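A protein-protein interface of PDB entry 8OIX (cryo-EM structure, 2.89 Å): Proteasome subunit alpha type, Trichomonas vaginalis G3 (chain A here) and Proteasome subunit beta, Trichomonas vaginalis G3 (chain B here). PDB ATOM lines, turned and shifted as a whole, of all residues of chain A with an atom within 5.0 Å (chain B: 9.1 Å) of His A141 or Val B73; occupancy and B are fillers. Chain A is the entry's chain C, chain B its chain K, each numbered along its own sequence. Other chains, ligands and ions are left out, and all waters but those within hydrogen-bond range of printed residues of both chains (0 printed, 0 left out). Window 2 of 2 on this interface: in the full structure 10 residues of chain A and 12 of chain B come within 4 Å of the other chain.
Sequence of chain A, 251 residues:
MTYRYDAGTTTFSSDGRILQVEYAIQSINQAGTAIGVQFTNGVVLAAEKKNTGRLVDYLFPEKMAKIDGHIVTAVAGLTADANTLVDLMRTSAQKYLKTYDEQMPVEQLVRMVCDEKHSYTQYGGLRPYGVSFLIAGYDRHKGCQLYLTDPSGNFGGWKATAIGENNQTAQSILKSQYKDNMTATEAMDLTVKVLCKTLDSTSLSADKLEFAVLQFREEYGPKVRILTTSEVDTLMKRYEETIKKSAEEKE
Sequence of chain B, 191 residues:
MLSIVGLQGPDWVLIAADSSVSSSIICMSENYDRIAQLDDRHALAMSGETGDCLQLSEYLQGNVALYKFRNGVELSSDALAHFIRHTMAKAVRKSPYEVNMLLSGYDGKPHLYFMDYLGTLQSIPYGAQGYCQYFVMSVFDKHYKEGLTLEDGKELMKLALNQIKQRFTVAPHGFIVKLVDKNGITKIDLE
The backbone carbonyl oxygen of Tyr B67 is in hydrogen-bond range of the side-chain amide nitrogen of Asn B71 (3.3 Å).
OE2 of Glu A102 is in salt-bridge range of NE of Arg A140.
OE2 of Glu A102 is in hydrogen-bond range of NE2 of His A141.
The backbone NH (N) of His A141 sits close to the side-chain carboxylate (OD1) of Asp A139 (3.1 Å).
Of the 18 printed residues of chain B, 6 touch a printed residue of chain A.
Along chain B the printed residues that touch a printed residue of chain A span positions 67 to 79.
Of the 8 printed residues of chain A, 5 touch a printed residue of chain B.
Among the printed residues, 10 pairs touch across the chains.
Among the printed residues, no Asp or Glu carboxylate lies within 4 Å of a Lys or Arg side-chain nitrogen of the other chain.
Glu A102 touches Ala B79 (OE1 to CB, 3.2 Å).
OH of Tyr B67 touches CG of Pro A105 (3.8 Å).
Gln A108 touches Val B73 (NE2 to CG2, 3.7 Å).
NH2 of Arg A140 touches O of Glu B74, at 3.7 Å.
Arg A140 touches Ser B76 (NH2 to CB, 3.4 Å).
NE2 of His A141 touches OH of Tyr B67, 3.97 Å away.
Val B73 touches His A141.
Glu B74 touches His A141 (O to CE1, 3.95 Å).
The side-chain hydroxyl (OH) of Tyr B67 lies within hydrogen-bond range of the side-chain amide nitrogen (NE2) of Gln A108 (2.8 Å).
ND2 of Asn B71 sits close to NE2 of Gln A108 (3.0 Å).
Of chain B, only Tyr B67 (3.97 Å), Val B73 (3.3 Å) and Glu B74 (3.95 Å) come within 4 Å of His A141.
Of chain A, only Gln A108 and His A141 come within 4 Å of Val B73.
Of the printed residues of chain A, Glu B74 touches Arg A140 and His A141.
Of the printed residues of chain A, Ser B76 touches Arg A140.
Of the printed residues of chain A, Ala B79 touches Glu A102 (3.2 Å).
The nearest residue of chain A that does not touch Val B73 is Lys A142 (4.4 Å).
The nearest printed residue of chain B that does not touch Glu A102 is Ser B76 (4.6 Å).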
ATOM      1  N   GLU A 102     -32.591 -14.001 -14.486  1.00  0.00           N
ATOM      2  CA  GLU A 102     -31.254 -13.631 -14.914  1.00  0.00           C
ATOM      3  C   GLU A 102     -31.357 -12.530 -15.956  1.00  0.00           C
ATOM      4  O   GLU A 102     -32.315 -12.478 -16.731  1.00  0.00           O
ATOM      5  CB  GLU A 102     -30.501 -14.852 -15.481  1.00  0.00           C
ATOM      6  CG  GLU A 102     -29.318 -14.524 -16.377  1.00  0.00           C
ATOM      7  CD  GLU A 102     -28.562 -15.755 -16.831  1.00  0.00           C
ATOM      8  OE1 GLU A 102     -29.072 -16.875 -16.627  1.00  0.00           O
ATOM      9  OE2 GLU A 102     -27.459 -15.602 -17.395  1.00  0.00           O
ATOM     10  N   PRO A 105     -28.906 -12.373 -21.762  1.00  0.00           N
ATOM     11  CA  PRO A 105     -27.622 -12.292 -22.460  1.00  0.00           C
ATOM     12  C   PRO A 105     -27.723 -11.350 -23.646  1.00  0.00           C
ATOM     13  O   PRO A 105     -28.743 -11.297 -24.335  1.00  0.00           O
ATOM     14  CB  PRO A 105     -27.368 -13.737 -22.899  1.00  0.00           C
ATOM     15  CG  PRO A 105     -28.095 -14.552 -21.890  1.00  0.00           C
ATOM     16  CD  PRO A 105     -29.338 -13.767 -21.572  1.00  0.00           C
ATOM     17  N   GLN A 108     -28.643 -12.675 -27.026  1.00  0.00           N
ATOM     18  CA  GLN A 108     -30.008 -13.149 -27.193  1.00  0.00           C
ATOM     19  C   GLN A 108     -30.976 -11.993 -27.388  1.00  0.00           C
ATOM     20  O   GLN A 108     -31.920 -12.103 -28.175  1.00  0.00           O
ATOM     21  CB  GLN A 108     -30.425 -13.976 -25.980  1.00  0.00           C
ATOM     22  CG  GLN A 108     -29.464 -15.090 -25.642  1.00  0.00           C
ATOM     23  CD  GLN A 108     -29.977 -15.970 -24.532  1.00  0.00           C
ATOM     24  OE1 GLN A 108     -31.115 -15.825 -24.090  1.00  0.00           O
ATOM     25  NE2 GLN A 108     -29.136 -16.881 -24.061  1.00  0.00           N
ATOM     26  N   ASP A 139     -23.001  -9.750 -20.392  1.00  0.00           N
ATOM     27  CA  ASP A 139     -23.570 -10.966 -19.834  1.00  0.00           C
ATOM     28  C   ASP A 139     -22.438 -11.865 -19.366  1.00  0.00           C
ATOM     29  O   ASP A 139     -21.331 -11.819 -19.903  1.00  0.00           O
ATOM     30  CB  ASP A 139     -24.479 -11.698 -20.833  1.00  0.00           C
ATOM     31  CG  ASP A 139     -23.767 -12.084 -22.111  1.00  0.00           C
ATOM     32  OD1 ASP A 139     -22.823 -12.900 -22.063  1.00  0.00           O
ATOM     33  OD2 ASP A 139     -24.159 -11.570 -23.178  1.00  0.00           O
ATOM     34  N   ARG A 140     -22.722 -12.658 -18.330  1.00  0.00           N
ATOM     35  CA  ARG A 140     -21.718 -13.563 -17.776  1.00  0.00           C
ATOM     36  C   ARG A 140     -21.103 -14.448 -18.854  1.00  0.00           C
ATOM     37  O   ARG A 140     -19.914 -14.779 -18.794  1.00  0.00           O
ATOM     38  CB  ARG A 140     -22.338 -14.408 -16.661  1.00  0.00           C
ATOM     39  CG  ARG A 140     -23.408 -15.383 -17.121  1.00  0.00           C
ATOM     40  CD  ARG A 140     -24.094 -16.047 -15.938  1.00  0.00           C
ATOM     41  NE  ARG A 140     -24.873 -17.219 -16.324  1.00  0.00           N
ATOM     42  CZ  ARG A 140     -24.362 -18.344 -16.803  1.00  0.00           C
ATOM     43  NH1 ARG A 140     -23.056 -18.506 -16.950  1.00  0.00           N
ATOM     44  NH2 ARG A 140     -25.179 -19.339 -17.135  1.00  0.00           N
ATOM     45  N   HIS A 141     -21.903 -14.842 -19.848  1.00  0.00           N
ATOM     46  CA  HIS A 141     -21.452 -15.808 -20.844  1.00  0.00           C
ATOM     47  C   HIS A 141     -20.286 -15.273 -21.666  1.00  0.00           C
ATOM     48  O   HIS A 141     -19.239 -15.920 -21.774  1.00  0.00           O
ATOM     49  CB  HIS A 141     -22.612 -16.175 -21.764  1.00  0.00           C
ATOM     50  CG  HIS A 141     -23.852 -16.596 -21.042  1.00  0.00           C
ATOM     51  ND1 HIS A 141     -24.016 -17.863 -20.524  1.00  0.00           N
ATOM     52  CD2 HIS A 141     -24.992 -15.923 -20.760  1.00  0.00           C
ATOM     53  CE1 HIS A 141     -25.203 -17.950 -19.951  1.00  0.00           C
ATOM     54  NE2 HIS A 141     -25.815 -16.787 -20.078  1.00  0.00           N
ATOM     55  N   LYS A 142     -20.451 -14.089 -22.256  1.00  0.00           N
ATOM     56  CA  LYS A 142     -19.489 -13.559 -23.216  1.00  0.00           C
ATOM     57  C   LYS A 142     -18.930 -12.207 -22.795  1.00  0.00           C
ATOM     58  O   LYS A 142     -18.470 -11.439 -23.646  1.00  0.00           O
ATOM     59  CB  LYS A 142     -20.124 -13.463 -24.604  1.00  0.00           C
ATOM     60  CG  LYS A 142     -20.502 -14.808 -25.205  1.00  0.00           C
ATOM     61  CD  LYS A 142     -21.305 -14.646 -26.482  1.00  0.00           C
ATOM     62  CE  LYS A 142     -22.766 -15.006 -26.265  1.00  0.00           C
ATOM     63  NZ  LYS A 142     -23.445 -14.068 -25.328  1.00  0.00           N
ATOM     64  N   GLY A 143     -18.952 -11.902 -21.500  1.00  0.00           N
ATOM     65  CA  GLY A 143     -18.403 -10.651 -21.029  1.00  0.00           C
ATOM     66  C   GLY A 143     -19.176  -9.463 -21.566  1.00  0.00           C
ATOM     67  O   GLY A 143     -20.399  -9.504 -21.749  1.00  0.00           O
ATOM     68  N   ASP B  39     -30.212 -31.521 -18.693  1.00  0.00           N
ATOM     69  CA  ASP B  39     -28.941 -31.161 -19.293  1.00  0.00           C
ATOM     70  C   ASP B  39     -27.904 -32.162 -18.799  1.00  0.00           C
ATOM     71  O   ASP B  39     -28.187 -33.005 -17.945  1.00  0.00           O
ATOM     72  CB  ASP B  39     -28.546 -29.721 -18.926  1.00  0.00           C
ATOM     73  CG  ASP B  39     -27.423 -29.178 -19.790  1.00  0.00           C
ATOM     74  OD1 ASP B  39     -26.311 -29.746 -19.756  1.00  0.00           O
ATOM     75  OD2 ASP B  39     -27.652 -28.177 -20.500  1.00  0.00           O
ATOM     76  N   ARG B  41     -25.641 -31.238 -17.018  1.00  0.00           N
ATOM     77  CA  ARG B  41     -25.334 -30.660 -15.721  1.00  0.00           C
ATOM     78  C   ARG B  41     -26.486 -30.734 -14.729  1.00  0.00           C
ATOM     79  O   ARG B  41     -26.247 -30.613 -13.525  1.00  0.00           O
ATOM     80  CB  ARG B  41     -24.924 -29.194 -15.902  1.00  0.00           C
ATOM     81  CG  ARG B  41     -23.558 -29.010 -16.536  1.00  0.00           C
ATOM     82  CD  ARG B  41     -23.511 -27.770 -17.415  1.00  0.00           C
ATOM     83  NE  ARG B  41     -23.938 -26.562 -16.720  1.00  0.00           N
ATOM     84  CZ  ARG B  41     -24.977 -25.821 -17.081  1.00  0.00           C
ATOM     85  NH1 ARG B  41     -25.852 -26.247 -17.976  1.00  0.00           N
ATOM     86  NH2 ARG B  41     -25.178 -24.651 -16.482  1.00  0.00           N
ATOM     87  N   ASN B  63     -36.558 -27.848 -23.953  1.00  0.00           N
ATOM     88  CA  ASN B  63     -36.353 -26.408 -23.848  1.00  0.00           C
ATOM     89  C   ASN B  63     -34.920 -26.072 -23.452  1.00  0.00           C
ATOM     90  O   ASN B  63     -34.359 -25.083 -23.930  1.00  0.00           O
ATOM     91  CB  ASN B  63     -37.343 -25.812 -22.852  1.00  0.00           C
ATOM     92  CG  ASN B  63     -38.707 -25.581 -23.461  1.00  0.00           C
ATOM     93  OD1 ASN B  63     -38.940 -24.571 -24.123  1.00  0.00           O
ATOM     94  ND2 ASN B  63     -39.617 -26.519 -23.242  1.00  0.00           N
ATOM     95  N   VAL B  64     -34.309 -26.878 -22.582  1.00  0.00           N
ATOM     96  CA  VAL B  64     -32.916 -26.649 -22.212  1.00  0.00           C
ATOM     97  C   VAL B  64     -32.006 -26.845 -23.416  1.00  0.00           C
ATOM     98  O   VAL B  64     -31.109 -26.034 -23.679  1.00  0.00           O
ATOM     99  CB  VAL B  64     -32.507 -27.567 -21.046  1.00  0.00           C
ATOM    100  CG1 VAL B  64     -31.012 -27.472 -20.801  1.00  0.00           C
ATOM    101  CG2 VAL B  64     -33.258 -27.189 -19.796  1.00  0.00           C
ATOM    102  N   ALA B  65     -32.227 -27.923 -24.171  1.00  0.00           N
ATOM    103  CA  ALA B  65     -31.432 -28.151 -25.370  1.00  0.00           C
ATOM    104  C   ALA B  65     -31.668 -27.050 -26.396  1.00  0.00           C
ATOM    105  O   ALA B  65     -30.733 -26.609 -27.072  1.00  0.00           O
ATOM    106  CB  ALA B  65     -31.750 -29.523 -25.960  1.00  0.00           C
ATOM    107  N   LEU B  66     -32.913 -26.588 -26.519  1.00  0.00           N
ATOM    108  CA  LEU B  66     -33.224 -25.522 -27.460  1.00  0.00           C
ATOM    109  C   LEU B  66     -32.560 -24.217 -27.049  1.00  0.00           C
ATOM    110  O   LEU B  66     -32.154 -23.437 -27.911  1.00  0.00           O
ATOM    111  CB  LEU B  66     -34.738 -25.349 -27.567  1.00  0.00           C
ATOM    112  CG  LEU B  66     -35.263 -24.281 -28.523  1.00  0.00           C
ATOM    113  CD1 LEU B  66     -34.793 -24.557 -29.935  1.00  0.00           C
ATOM    114  CD2 LEU B  66     -36.779 -24.219 -28.463  1.00  0.00           C
ATOM    115  N   TYR B  67     -32.456 -23.954 -25.746  1.00  0.00           N
ATOM    116  CA  TYR B  67     -31.727 -22.777 -25.288  1.00  0.00           C
ATOM    117  C   TYR B  67     -30.238 -22.925 -25.574  1.00  0.00           C
ATOM    118  O   TYR B  67     -29.569 -21.956 -25.946  1.00  0.00           O
ATOM    119  CB  TYR B  67     -31.976 -22.556 -23.795  1.00  0.00           C
ATOM    120  CG  TYR B  67     -31.241 -21.374 -23.204  1.00  0.00           C
ATOM    121  CD1 TYR B  67     -29.940 -21.497 -22.735  1.00  0.00           C
ATOM    122  CD2 TYR B  67     -31.858 -20.135 -23.101  1.00  0.00           C
ATOM    123  CE1 TYR B  67     -29.272 -20.419 -22.195  1.00  0.00           C
ATOM    124  CE2 TYR B  67     -31.197 -19.052 -22.559  1.00  0.00           C
ATOM    125  CZ  TYR B  67     -29.905 -19.199 -22.108  1.00  0.00           C
ATOM    126  OH  TYR B  67     -29.243 -18.124 -21.567  1.00  0.00           O
ATOM    127  N   LYS B  68     -29.706 -24.137 -25.398  1.00  0.00           N
ATOM    128  CA  LYS B  68     -28.291 -24.388 -25.650  1.00  0.00           C
ATOM    129  C   LYS B  68     -27.952 -24.260 -27.129  1.00  0.00           C
ATOM    130  O   LYS B  68     -26.816 -23.922 -27.480  1.00  0.00           O
ATOM    131  CB  LYS B  68     -27.909 -25.780 -25.145  1.00  0.00           C
ATOM    132  CG  LYS B  68     -26.454 -26.150 -25.367  1.00  0.00           C
ATOM    133  CD  LYS B  68     -26.172 -27.564 -24.900  1.00  0.00           C
ATOM    134  CE  LYS B  68     -26.919 -28.576 -25.748  1.00  0.00           C
ATOM    135  NZ  LYS B  68     -26.620 -29.973 -25.338  1.00  0.00           N
ATOM    136  N   PHE B  69     -28.904 -24.564 -28.004  1.00  0.00           N
ATOM    137  CA  PHE B  69     -28.658 -24.540 -29.439  1.00  0.00           C
ATOM    138  C   PHE B  69     -28.982 -23.183 -30.055  1.00  0.00           C
ATOM    139  O   PHE B  69     -28.240 -22.705 -30.919  1.00  0.00           O
ATOM    140  CB  PHE B  69     -29.453 -25.661 -30.106  1.00  0.00           C
ATOM    141  CG  PHE B  69     -28.934 -27.026 -29.770  1.00  0.00           C
ATOM    142  CD1 PHE B  69     -27.573 -27.251 -29.675  1.00  0.00           C
ATOM    143  CD2 PHE B  69     -29.799 -28.068 -29.495  1.00  0.00           C
ATOM    144  CE1 PHE B  69     -27.084 -28.496 -29.346  1.00  0.00           C
ATOM    145  CE2 PHE B  69     -29.315 -29.313 -29.156  1.00  0.00           C
ATOM    146  CZ  PHE B  69     -27.955 -29.528 -29.086  1.00  0.00           C
ATOM    147  N   ARG B  70     -30.082 -22.559 -29.629  1.00  0.00           N
ATOM    148  CA  ARG B  70     -30.423 -21.219 -30.094  1.00  0.00           C
ATOM    149  C   ARG B  70     -29.329 -20.231 -29.725  1.00  0.00           C
ATOM    150  O   ARG B  70     -28.862 -19.451 -30.563  1.00  0.00           O
ATOM    151  CB  ARG B  70     -31.749 -20.782 -29.471  1.00  0.00           C
ATOM    152  CG  ARG B  70     -32.987 -21.352 -30.117  1.00  0.00           C
ATOM    153  CD  ARG B  70     -33.298 -20.605 -31.388  1.00  0.00           C
ATOM    154  NE  ARG B  70     -33.694 -19.228 -31.119  1.00  0.00           N
ATOM    155  CZ  ARG B  70     -34.803 -18.872 -30.484  1.00  0.00           C
ATOM    156  NH1 ARG B  70     -35.771 -19.741 -30.240  1.00  0.00           N
ATOM    157  NH2 ARG B  70     -34.978 -17.596 -30.152  1.00  0.00           N
ATOM    158  N   ASN B  71     -28.907 -20.260 -28.470  1.00  0.00           N
ATOM    159  CA  ASN B  71     -27.838 -19.426 -27.957  1.00  0.00           C
ATOM    160  C   ASN B  71     -26.685 -20.338 -27.575  1.00  0.00           C
ATOM    161  O   ASN B  71     -26.898 -21.381 -26.954  1.00  0.00           O
ATOM    162  CB  ASN B  71     -28.317 -18.633 -26.743  1.00  0.00           C
ATOM    163  CG  ASN B  71     -29.788 -18.282 -26.831  1.00  0.00           C
ATOM    164  OD1 ASN B  71     -30.214 -17.561 -27.733  1.00  0.00           O
ATOM    165  ND2 ASN B  71     -30.577 -18.802 -25.899  1.00  0.00           N
ATOM    166  N   GLY B  72     -25.463 -19.940 -27.904  1.00  0.00           N
ATOM    167  CA  GLY B  72     -24.358 -20.855 -27.693  1.00  0.00           C
ATOM    168  C   GLY B  72     -23.908 -20.882 -26.249  1.00  0.00           C
ATOM    169  O   GLY B  72     -22.708 -20.870 -25.955  1.00  0.00           O
ATOM    170  N   VAL B  73     -24.879 -20.934 -25.339  1.00  0.00           N
ATOM    171  CA  VAL B  73     -24.642 -20.916 -23.902  1.00  0.00           C
ATOM    172  C   VAL B  73     -25.649 -21.845 -23.239  1.00  0.00           C
ATOM    173  O   VAL B  73     -26.810 -21.920 -23.655  1.00  0.00           O
ATOM    174  CB  VAL B  73     -24.743 -19.488 -23.326  1.00  0.00           C
ATOM    175  CG1 VAL B  73     -23.668 -18.603 -23.920  1.00  0.00           C
ATOM    176  CG2 VAL B  73     -26.119 -18.895 -23.592  1.00  0.00           C
ATOM    177  N   GLU B  74     -25.200 -22.570 -22.221  1.00  0.00           N
ATOM    178  CA  GLU B  74     -26.079 -23.441 -21.458  1.00  0.00           C
ATOM    179  C   GLU B  74     -26.703 -22.685 -20.294  1.00  0.00           C
ATOM    180  O   GLU B  74     -26.085 -21.794 -19.703  1.00  0.00           O
ATOM    181  CB  GLU B  74     -25.316 -24.659 -20.937  1.00  0.00           C
ATOM    182  CG  GLU B  74     -24.993 -25.690 -22.001  1.00  0.00           C
ATOM    183  CD  GLU B  74     -24.267 -26.895 -21.441  1.00  0.00           C
ATOM    184  OE1 GLU B  74     -23.158 -26.723 -20.896  1.00  0.00           O
ATOM    185  OE2 GLU B  74     -24.809 -28.016 -21.545  1.00  0.00           O
ATOM    186  N   LEU B  75     -27.947 -23.040 -19.979  1.00  0.00           N
ATOM    187  CA  LEU B  75     -28.634 -22.430 -18.851  1.00  0.00           C
ATOM    188  C   LEU B  75     -27.882 -22.694 -17.553  1.00  0.00           C
ATOM    189  O   LEU B  75     -27.280 -23.753 -17.362  1.00  0.00           O
ATOM    190  CB  LEU B  75     -30.060 -22.971 -18.728  1.00  0.00           C
ATOM    191  CG  LEU B  75     -31.155 -22.359 -19.598  1.00  0.00           C
ATOM    192  CD1 LEU B  75     -32.458 -23.114 -19.412  1.00  0.00           C
ATOM    193  CD2 LEU B  75     -31.331 -20.892 -19.261  1.00  0.00           C
ATOM    194  N   SER B  76     -27.918 -21.713 -16.657  1.00  0.00           N
ATOM    195  CA  SER B  76     -27.346 -21.896 -15.335  1.00  0.00           C
ATOM    196  C   SER B  76     -28.265 -22.796 -14.512  1.00  0.00           C
ATOM    197  O   SER B  76     -29.289 -23.287 -14.992  1.00  0.00           O
ATOM    198  CB  SER B  76     -27.139 -20.545 -14.655  1.00  0.00           C
ATOM    199  OG  SER B  76     -26.456 -20.690 -13.423  1.00  0.00           O
ATOM    200  N   SER B  77     -27.907 -23.017 -13.249  1.00  0.00           N
ATOM    201  CA  SER B  77     -28.825 -23.747 -12.386  1.00  0.00           C
ATOM    202  C   SER B  77     -29.896 -22.831 -11.819  1.00  0.00           C
ATOM    203  O   SER B  77     -31.041 -23.259 -11.652  1.00  0.00           O
ATOM    204  CB  SER B  77     -28.069 -24.439 -11.254  1.00  0.00           C
ATOM    205  OG  SER B  77     -27.235 -25.466 -11.757  1.00  0.00           O
ATOM    206  N   ALA B  79     -30.903 -20.075 -13.524  1.00  0.00           N
ATOM    207  CA  ALA B  79     -31.709 -19.772 -14.700  1.00  0.00           C
ATOM    208  C   ALA B  79     -32.623 -20.936 -15.056  1.00  0.00           C
ATOM    209  O   ALA B  79     -33.809 -20.736 -15.338  1.00  0.00           O
ATOM    210  CB  ALA B  79     -30.806 -19.419 -15.880  1.00  0.00           C
